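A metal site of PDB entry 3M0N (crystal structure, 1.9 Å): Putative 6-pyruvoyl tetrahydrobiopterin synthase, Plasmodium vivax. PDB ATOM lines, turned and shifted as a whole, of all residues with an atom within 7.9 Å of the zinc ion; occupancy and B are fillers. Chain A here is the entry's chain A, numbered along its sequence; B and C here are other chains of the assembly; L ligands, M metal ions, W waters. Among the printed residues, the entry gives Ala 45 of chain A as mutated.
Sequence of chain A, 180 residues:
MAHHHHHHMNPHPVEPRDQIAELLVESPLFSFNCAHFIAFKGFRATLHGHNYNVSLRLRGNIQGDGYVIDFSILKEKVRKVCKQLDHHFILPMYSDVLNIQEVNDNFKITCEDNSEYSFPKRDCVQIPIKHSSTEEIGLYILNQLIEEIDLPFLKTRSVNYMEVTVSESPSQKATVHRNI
A nitrogen (N5) of the ligand lies close to the side-chain carboxylate (OE2) of Glu 168, 3.2 Å away.
An oxygen (O1) of the ligand is in hydrogen-bond range of the backbone NH (N) of Thr 134.
The side-chain hydroxyl (OG1) of Thr 134 lies within hydrogen-bond range of an oxygen (O1) of the ligand (3.0 Å).
ND1 of His 50 lies close to O of Glu 168 (3.5 Å).
ND1 of His 50 lies within hydrogen-bond range of OD1 of Asn 51 of chain B (3.0 Å).
The backbone carbonyl oxygen of Cys 34 sits at hydrogen-bond distance from the backbone NH of His 50.
A ring nitrogen (ND1) of His 48 lies within hydrogen-bond range of the backbone carbonyl oxygen (O) of Thr 46, at 2.8 Å.
A ring nitrogen (ND1) of His 36 sits at hydrogen-bond distance from the side-chain hydroxyl (OG) of Ser 132 (2.9 Å).
The side-chain amide nitrogen (NE2) of Gln 172 lies within hydrogen-bond range of the side-chain carboxylate (OE1) of Glu 168, at 2.7 Å.
O of Glu 168 lies within hydrogen-bond range of ND2 of Asn 51 of chain B (2.9 Å).
OE2 of Glu 168 touches the zinc ion, at 3.2 Å.
Four residues have an atom within 4 Å of the zinc ion: His 36, His 48, His 50 and Glu 168.
The nearest printed residue that does not touch the zinc ion is His 87 of chain B (4.7 Å).
The zinc ion is bound by a ring nitrogen (NE2) of His 50 (2.0 Å), a ring nitrogen (NE2) of His 48 (2.0 Å) and a ring nitrogen (NE2) of His 36 (2.1 Å).
The zinc ion has three donor atoms within binding distance.
Slightly farther from the zinc ion lies water W1 (2.6 Å).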
ATOM      1  N   CYS A  34     -22.668  -9.810 -27.936  1.00  0.00           N
ATOM      2  CA  CYS A  34     -21.795  -8.774 -28.465  1.00  0.00           C
ATOM      3  C   CYS A  34     -21.597  -7.608 -27.495  1.00  0.00           C
ATOM      4  O   CYS A  34     -22.440  -7.370 -26.617  1.00  0.00           O
ATOM      5  CB  CYS A  34     -22.409  -8.228 -29.764  1.00  0.00           C
ATOM      6  SG  CYS A  34     -22.314  -9.406 -31.145  1.00  0.00           S
ATOM      7  N   ALA A  35     -20.485  -6.894 -27.680  1.00  0.00           N
ATOM      8  CA  ALA A  35     -20.237  -5.633 -27.008  1.00  0.00           C
ATOM      9  C   ALA A  35     -20.631  -4.527 -27.970  1.00  0.00           C
ATOM     10  O   ALA A  35     -20.574  -4.711 -29.188  1.00  0.00           O
ATOM     11  CB  ALA A  35     -18.750  -5.495 -26.626  1.00  0.00           C
ATOM     12  N   HIS A  36     -20.994  -3.370 -27.415  1.00  0.00           N
ATOM     13  CA  HIS A  36     -21.293  -2.186 -28.253  1.00  0.00           C
ATOM     14  C   HIS A  36     -21.336  -0.963 -27.344  1.00  0.00           C
ATOM     15  O   HIS A  36     -21.169  -1.083 -26.129  1.00  0.00           O
ATOM     16  CB  HIS A  36     -22.589  -2.368 -29.007  1.00  0.00           C
ATOM     17  CG  HIS A  36     -23.823  -1.928 -28.263  1.00  0.00           C
ATOM     18  ND1 HIS A  36     -24.729  -1.044 -28.807  1.00  0.00           N
ATOM     19  CD2 HIS A  36     -24.301  -2.272 -27.050  1.00  0.00           C
ATOM     20  CE1 HIS A  36     -25.711  -0.851 -27.942  1.00  0.00           C
ATOM     21  NE2 HIS A  36     -25.476  -1.585 -26.868  1.00  0.00           N
ATOM     22  N   PHE A  37     -21.478   0.201 -27.932  1.00  0.00           N
ATOM     23  CA  PHE A  37     -21.886   1.341 -27.166  1.00  0.00           C
ATOM     24  C   PHE A  37     -22.653   2.251 -28.087  1.00  0.00           C
ATOM     25  O   PHE A  37     -22.354   2.316 -29.264  1.00  0.00           O
ATOM     26  CB  PHE A  37     -20.714   2.066 -26.425  1.00  0.00           C
ATOM     27  CG  PHE A  37     -19.665   2.734 -27.334  1.00  0.00           C
ATOM     28  CD1 PHE A  37     -19.883   4.017 -27.856  1.00  0.00           C
ATOM     29  CD2 PHE A  37     -18.425   2.132 -27.553  1.00  0.00           C
ATOM     30  CE1 PHE A  37     -18.902   4.658 -28.639  1.00  0.00           C
ATOM     31  CE2 PHE A  37     -17.435   2.764 -28.320  1.00  0.00           C
ATOM     32  CZ  PHE A  37     -17.678   4.020 -28.871  1.00  0.00           C
ATOM     33  N   ILE A  38     -23.625   2.944 -27.521  1.00  0.00           N
ATOM     34  CA  ILE A  38     -24.466   3.899 -28.254  1.00  0.00           C
ATOM     35  C   ILE A  38     -23.780   5.255 -28.283  1.00  0.00           C
ATOM     36  O   ILE A  38     -23.278   5.709 -27.259  1.00  0.00           O
ATOM     37  CB  ILE A  38     -25.840   4.080 -27.550  1.00  0.00           C
ATOM     38  CG1 ILE A  38     -26.593   2.747 -27.495  1.00  0.00           C
ATOM     39  CG2 ILE A  38     -26.696   5.137 -28.277  1.00  0.00           C
ATOM     40  CD1 ILE A  38     -26.864   2.150 -28.870  1.00  0.00           C
ATOM     41  N   ALA A  45     -22.727   6.377 -24.642  1.00  0.00           N
ATOM     42  CA  ALA A  45     -22.860   5.400 -23.546  1.00  0.00           C
ATOM     43  C   ALA A  45     -21.505   4.777 -23.296  1.00  0.00           C
ATOM     44  O   ALA A  45     -20.654   4.733 -24.177  1.00  0.00           O
ATOM     45  CB  ALA A  45     -23.848   4.307 -23.901  1.00  0.00           C
ATOM     46  N   THR A  46     -21.315   4.291 -22.084  1.00  0.00           N
ATOM     47  CA  THR A  46     -20.131   3.501 -21.772  1.00  0.00           C
ATOM     48  C   THR A  46     -20.186   2.159 -22.540  1.00  0.00           C
ATOM     49  O   THR A  46     -21.253   1.676 -22.944  1.00  0.00           O
ATOM     50  CB  THR A  46     -20.016   3.256 -20.264  1.00  0.00           C
ATOM     51  OG1 THR A  46     -21.291   2.841 -19.748  1.00  0.00           O
ATOM     52  CG2 THR A  46     -19.620   4.524 -19.527  1.00  0.00           C
ATOM     53  N   LEU A  47     -19.019   1.556 -22.705  1.00  0.00           N
ATOM     54  CA  LEU A  47     -18.918   0.234 -23.303  1.00  0.00           C
ATOM     55  C   LEU A  47     -19.605  -0.821 -22.447  1.00  0.00           C
ATOM     56  O   LEU A  47     -19.432  -0.873 -21.233  1.00  0.00           O
ATOM     57  CB  LEU A  47     -17.451  -0.152 -23.454  1.00  0.00           C
ATOM     58  CG  LEU A  47     -17.170  -1.528 -24.083  1.00  0.00           C
ATOM     59  CD1 LEU A  47     -17.637  -1.524 -25.538  1.00  0.00           C
ATOM     60  CD2 LEU A  47     -15.680  -1.815 -23.965  1.00  0.00           C
ATOM     61  N   HIS A  48     -20.387  -1.673 -23.111  1.00  0.00           N
ATOM     62  CA  HIS A  48     -21.125  -2.729 -22.436  1.00  0.00           C
ATOM     63  C   HIS A  48     -21.468  -3.777 -23.473  1.00  0.00           C
ATOM     64  O   HIS A  48     -20.830  -3.821 -24.519  1.00  0.00           O
ATOM     65  CB  HIS A  48     -22.368  -2.153 -21.734  1.00  0.00           C
ATOM     66  CG  HIS A  48     -23.390  -1.553 -22.661  1.00  0.00           C
ATOM     67  ND1 HIS A  48     -23.306  -0.257 -23.126  1.00  0.00           N
ATOM     68  CD2 HIS A  48     -24.536  -2.066 -23.155  1.00  0.00           C
ATOM     69  CE1 HIS A  48     -24.352  -0.007 -23.889  1.00  0.00           C
ATOM     70  NE2 HIS A  48     -25.120  -1.081 -23.913  1.00  0.00           N
ATOM     71  N   GLY A  49     -22.466  -4.616 -23.195  1.00  0.00           N
ATOM     72  CA  GLY A  49     -22.817  -5.694 -24.101  1.00  0.00           C
ATOM     73  C   GLY A  49     -24.179  -6.284 -23.814  1.00  0.00           C
ATOM     74  O   GLY A  49     -24.839  -5.918 -22.831  1.00  0.00           O
ATOM     75  N   HIS A  50     -24.587  -7.200 -24.679  1.00  0.00           N
ATOM     76  CA  HIS A  50     -25.904  -7.847 -24.636  1.00  0.00           C
ATOM     77  C   HIS A  50     -25.878  -9.234 -25.256  1.00  0.00           C
ATOM     78  O   HIS A  50     -25.056  -9.513 -26.135  1.00  0.00           O
ATOM     79  CB  HIS A  50     -26.947  -7.049 -25.428  1.00  0.00           C
ATOM     80  CG  HIS A  50     -27.106  -5.635 -24.990  1.00  0.00           C
ATOM     81  ND1 HIS A  50     -27.715  -5.279 -23.806  1.00  0.00           N
ATOM     82  CD2 HIS A  50     -26.779  -4.478 -25.614  1.00  0.00           C
ATOM     83  CE1 HIS A  50     -27.725  -3.967 -23.699  1.00  0.00           C
ATOM     84  NE2 HIS A  50     -27.178  -3.453 -24.781  1.00  0.00           N
ATOM     85  N   TYR A  52     -28.008 -10.516 -27.634  1.00  0.00           N
ATOM     86  CA  TYR A  52     -29.057 -10.140 -28.578  1.00  0.00           C
ATOM     87  C   TYR A  52     -29.755 -11.401 -29.006  1.00  0.00           C
ATOM     88  O   TYR A  52     -29.123 -12.443 -29.148  1.00  0.00           O
ATOM     89  CB  TYR A  52     -28.463  -9.460 -29.806  1.00  0.00           C
ATOM     90  CG  TYR A  52     -27.895  -8.082 -29.585  1.00  0.00           C
ATOM     91  CD1 TYR A  52     -28.660  -6.943 -29.831  1.00  0.00           C
ATOM     92  CD2 TYR A  52     -26.569  -7.911 -29.182  1.00  0.00           C
ATOM     93  CE1 TYR A  52     -28.129  -5.684 -29.674  1.00  0.00           C
ATOM     94  CE2 TYR A  52     -26.031  -6.639 -29.008  1.00  0.00           C
ATOM     95  CZ  TYR A  52     -26.827  -5.528 -29.253  1.00  0.00           C
ATOM     96  OH  TYR A  52     -26.307  -4.257 -29.095  1.00  0.00           O
ATOM     97  N   SER A 132     -25.314   1.447 -33.472  1.00  0.00           N
ATOM     98  CA  SER A 132     -25.534   0.080 -33.038  1.00  0.00           C
ATOM     99  C   SER A 132     -26.824  -0.022 -32.190  1.00  0.00           C
ATOM    100  O   SER A 132     -26.826  -0.626 -31.097  1.00  0.00           O
ATOM    101  CB  SER A 132     -24.301  -0.475 -32.283  1.00  0.00           C
ATOM    102  OG  SER A 132     -23.916   0.356 -31.195  1.00  0.00           O
ATOM    103  N   SER A 133     -27.916   0.574 -32.674  1.00  0.00           N
ATOM    104  CA  SER A 133     -29.218   0.427 -32.069  1.00  0.00           C
ATOM    105  C   SER A 133     -29.912  -0.849 -32.535  1.00  0.00           C
ATOM    106  O   SER A 133     -29.632  -1.386 -33.614  1.00  0.00           O
ATOM    107  CB  SER A 133     -30.125   1.628 -32.405  1.00  0.00           C
ATOM    108  OG  SER A 133     -30.429   1.652 -33.783  1.00  0.00           O
ATOM    109  N   THR A 134     -30.865  -1.288 -31.737  1.00  0.00           N
ATOM    110  CA  THR A 134     -31.673  -2.452 -32.041  1.00  0.00           C
ATOM    111  C   THR A 134     -32.410  -2.322 -33.368  1.00  0.00           C
ATOM    112  O   THR A 134     -32.484  -3.261 -34.139  1.00  0.00           O
ATOM    113  CB  THR A 134     -32.673  -2.647 -30.895  1.00  0.00           C
ATOM    114  OG1 THR A 134     -31.947  -2.714 -29.667  1.00  0.00           O
ATOM    115  CG2 THR A 134     -33.456  -3.900 -31.100  1.00  0.00           C
ATOM    116  N   GLU A 168     -32.526  -6.555 -27.557  1.00  0.00           N
ATOM    117  CA  GLU A 168     -31.301  -6.241 -26.812  1.00  0.00           C
ATOM    118  C   GLU A 168     -31.258  -6.995 -25.484  1.00  0.00           C
ATOM    119  O   GLU A 168     -30.195  -7.399 -25.009  1.00  0.00           O
ATOM    120  CB  GLU A 168     -31.239  -4.749 -26.504  1.00  0.00           C
ATOM    121  CG  GLU A 168     -30.134  -3.968 -27.206  1.00  0.00           C
ATOM    122  CD  GLU A 168     -30.078  -2.517 -26.723  1.00  0.00           C
ATOM    123  OE1 GLU A 168     -30.983  -2.137 -25.944  1.00  0.00           O
ATOM    124  OE2 GLU A 168     -29.138  -1.777 -27.121  1.00  0.00           O
ATOM    125  N   GLN A 172     -36.874  -5.363 -24.250  1.00  0.00           N
ATOM    126  CA  GLN A 172     -36.867  -4.317 -25.296  1.00  0.00           C
ATOM    127  C   GLN A 172     -36.505  -4.890 -26.654  1.00  0.00           C
ATOM    128  O   GLN A 172     -35.424  -5.460 -26.828  1.00  0.00           O
ATOM    129  CB  GLN A 172     -35.962  -3.121 -24.935  1.00  0.00           C
ATOM    130  CG  GLN A 172     -34.796  -3.415 -23.995  1.00  0.00           C
ATOM    131  CD  GLN A 172     -34.084  -2.148 -23.519  1.00  0.00           C
ATOM    132  OE1 GLN A 172     -34.669  -1.322 -22.805  1.00  0.00           O
ATOM    133  NE2 GLN A 172     -32.815  -2.000 -23.907  1.00  0.00           N
ATOM    134  N   ASN B  33     -25.673  -5.444 -17.852  1.00  0.00           N
ATOM    135  CA  ASN B  33     -25.370  -5.623 -19.247  1.00  0.00           C
ATOM    136  C   ASN B  33     -23.934  -5.136 -19.471  1.00  0.00           C
ATOM    137  O   ASN B  33     -23.692  -3.919 -19.501  1.00  0.00           O
ATOM    138  CB  ASN B  33     -26.400  -4.862 -20.083  1.00  0.00           C
ATOM    139  CG  ASN B  33     -27.843  -5.351 -19.830  1.00  0.00           C
ATOM    140  OD1 ASN B  33     -28.083  -6.381 -19.177  1.00  0.00           O
ATOM    141  ND2 ASN B  33     -28.802  -4.608 -20.365  1.00  0.00           N
ATOM    142  N   ASN B  51     -26.066  -9.979 -21.137  1.00  0.00           N
ATOM    143  CA  ASN B  51     -27.034  -9.555 -20.151  1.00  0.00           C
ATOM    144  C   ASN B  51     -26.921 -10.542 -19.020  1.00  0.00           C
ATOM    145  O   ASN B  51     -27.571 -11.590 -19.031  1.00  0.00           O
ATOM    146  CB  ASN B  51     -28.464  -9.560 -20.707  1.00  0.00           C
ATOM    147  CG  ASN B  51     -28.614  -8.682 -21.922  1.00  0.00           C
ATOM    148  OD1 ASN B  51     -28.078  -7.573 -21.966  1.00  0.00           O
ATOM    149  ND2 ASN B  51     -29.345  -9.155 -22.931  1.00  0.00           N
ATOM    150  N   HIS B  87     -23.604  -1.740 -17.517  1.00  0.00           N
ATOM    151  CA  HIS B  87     -23.081  -0.813 -18.528  1.00  0.00           C
ATOM    152  C   HIS B  87     -21.570  -0.507 -18.421  1.00  0.00           C
ATOM    153  O   HIS B  87     -21.144   0.624 -18.649  1.00  0.00           O
ATOM    154  CB  HIS B  87     -23.952   0.450 -18.596  1.00  0.00           C
ATOM    155  CG  HIS B  87     -25.153   0.306 -19.486  1.00  0.00           C
ATOM    156  ND1 HIS B  87     -25.490   1.231 -20.448  1.00  0.00           N
ATOM    157  CD2 HIS B  87     -26.057  -0.702 -19.588  1.00  0.00           C
ATOM    158  CE1 HIS B  87     -26.572   0.822 -21.086  1.00  0.00           C
ATOM    159  NE2 HIS B  87     -26.941  -0.344 -20.585  1.00  0.00           N
ATOM    160  N   TYR C  67     -32.838   5.765 -32.941  1.00  0.00           N
ATOM    161  CA  TYR C  67     -34.010   5.240 -32.226  1.00  0.00           C
ATOM    162  C   TYR C  67     -35.321   5.715 -32.880  1.00  0.00           C
ATOM    163  O   TYR C  67     -35.356   6.814 -33.425  1.00  0.00           O
ATOM    164  CB  TYR C  67     -34.022   5.784 -30.813  1.00  0.00           C
ATOM    165  CG  TYR C  67     -32.860   5.451 -29.907  1.00  0.00           C
ATOM    166  CD1 TYR C  67     -32.017   4.359 -30.148  1.00  0.00           C
ATOM    167  CD2 TYR C  67     -32.630   6.215 -28.758  1.00  0.00           C
ATOM    168  CE1 TYR C  67     -30.973   4.063 -29.269  1.00  0.00           C
ATOM    169  CE2 TYR C  67     -31.595   5.928 -27.894  1.00  0.00           C
ATOM    170  CZ  TYR C  67     -30.770   4.845 -28.146  1.00  0.00           C
ATOM    171  OH  TYR C  67     -29.753   4.558 -27.273  1.00  0.00           O
HETATM  172  C1  LIG L   1     -31.654   1.447 -27.365  1.00  0.00           C
HETATM  173  C2  LIG L   1     -31.978   0.987 -28.652  1.00  0.00           C
HETATM  174  O1  LIG L   1     -31.238   0.212 -29.279  1.00  0.00           O
HETATM  175  N1  LIG L   1     -33.152   1.437 -29.243  1.00  0.00           N
HETATM  176  C3  LIG L   1     -33.992   2.326 -28.554  1.00  0.00           C
HETATM  177  N2  LIG L   1     -35.119   2.746 -29.126  1.00  0.00           N
HETATM  178  N3  LIG L   1     -33.664   2.749 -27.306  1.00  0.00           N
HETATM  179  C4  LIG L   1     -32.517   2.329 -26.719  1.00  0.00           C
HETATM  180  N4  LIG L   1     -32.207   2.760 -25.482  1.00  0.00           N
HETATM  181  C5  LIG L   1     -31.090   2.352 -24.884  1.00  0.00           C
HETATM  182  C6  LIG L   1     -30.231   1.475 -25.537  1.00  0.00           C
HETATM  183  N5  LIG L   1     -30.518   1.039 -26.752  1.00  0.00           N
HETATM  184 ZN    ZN M   1     -26.644  -1.573 -25.093  1.00  0.00          ZN
HETATM  185  O   HOH W   1     -28.556  -0.222 -23.949  1.00  0.00           O
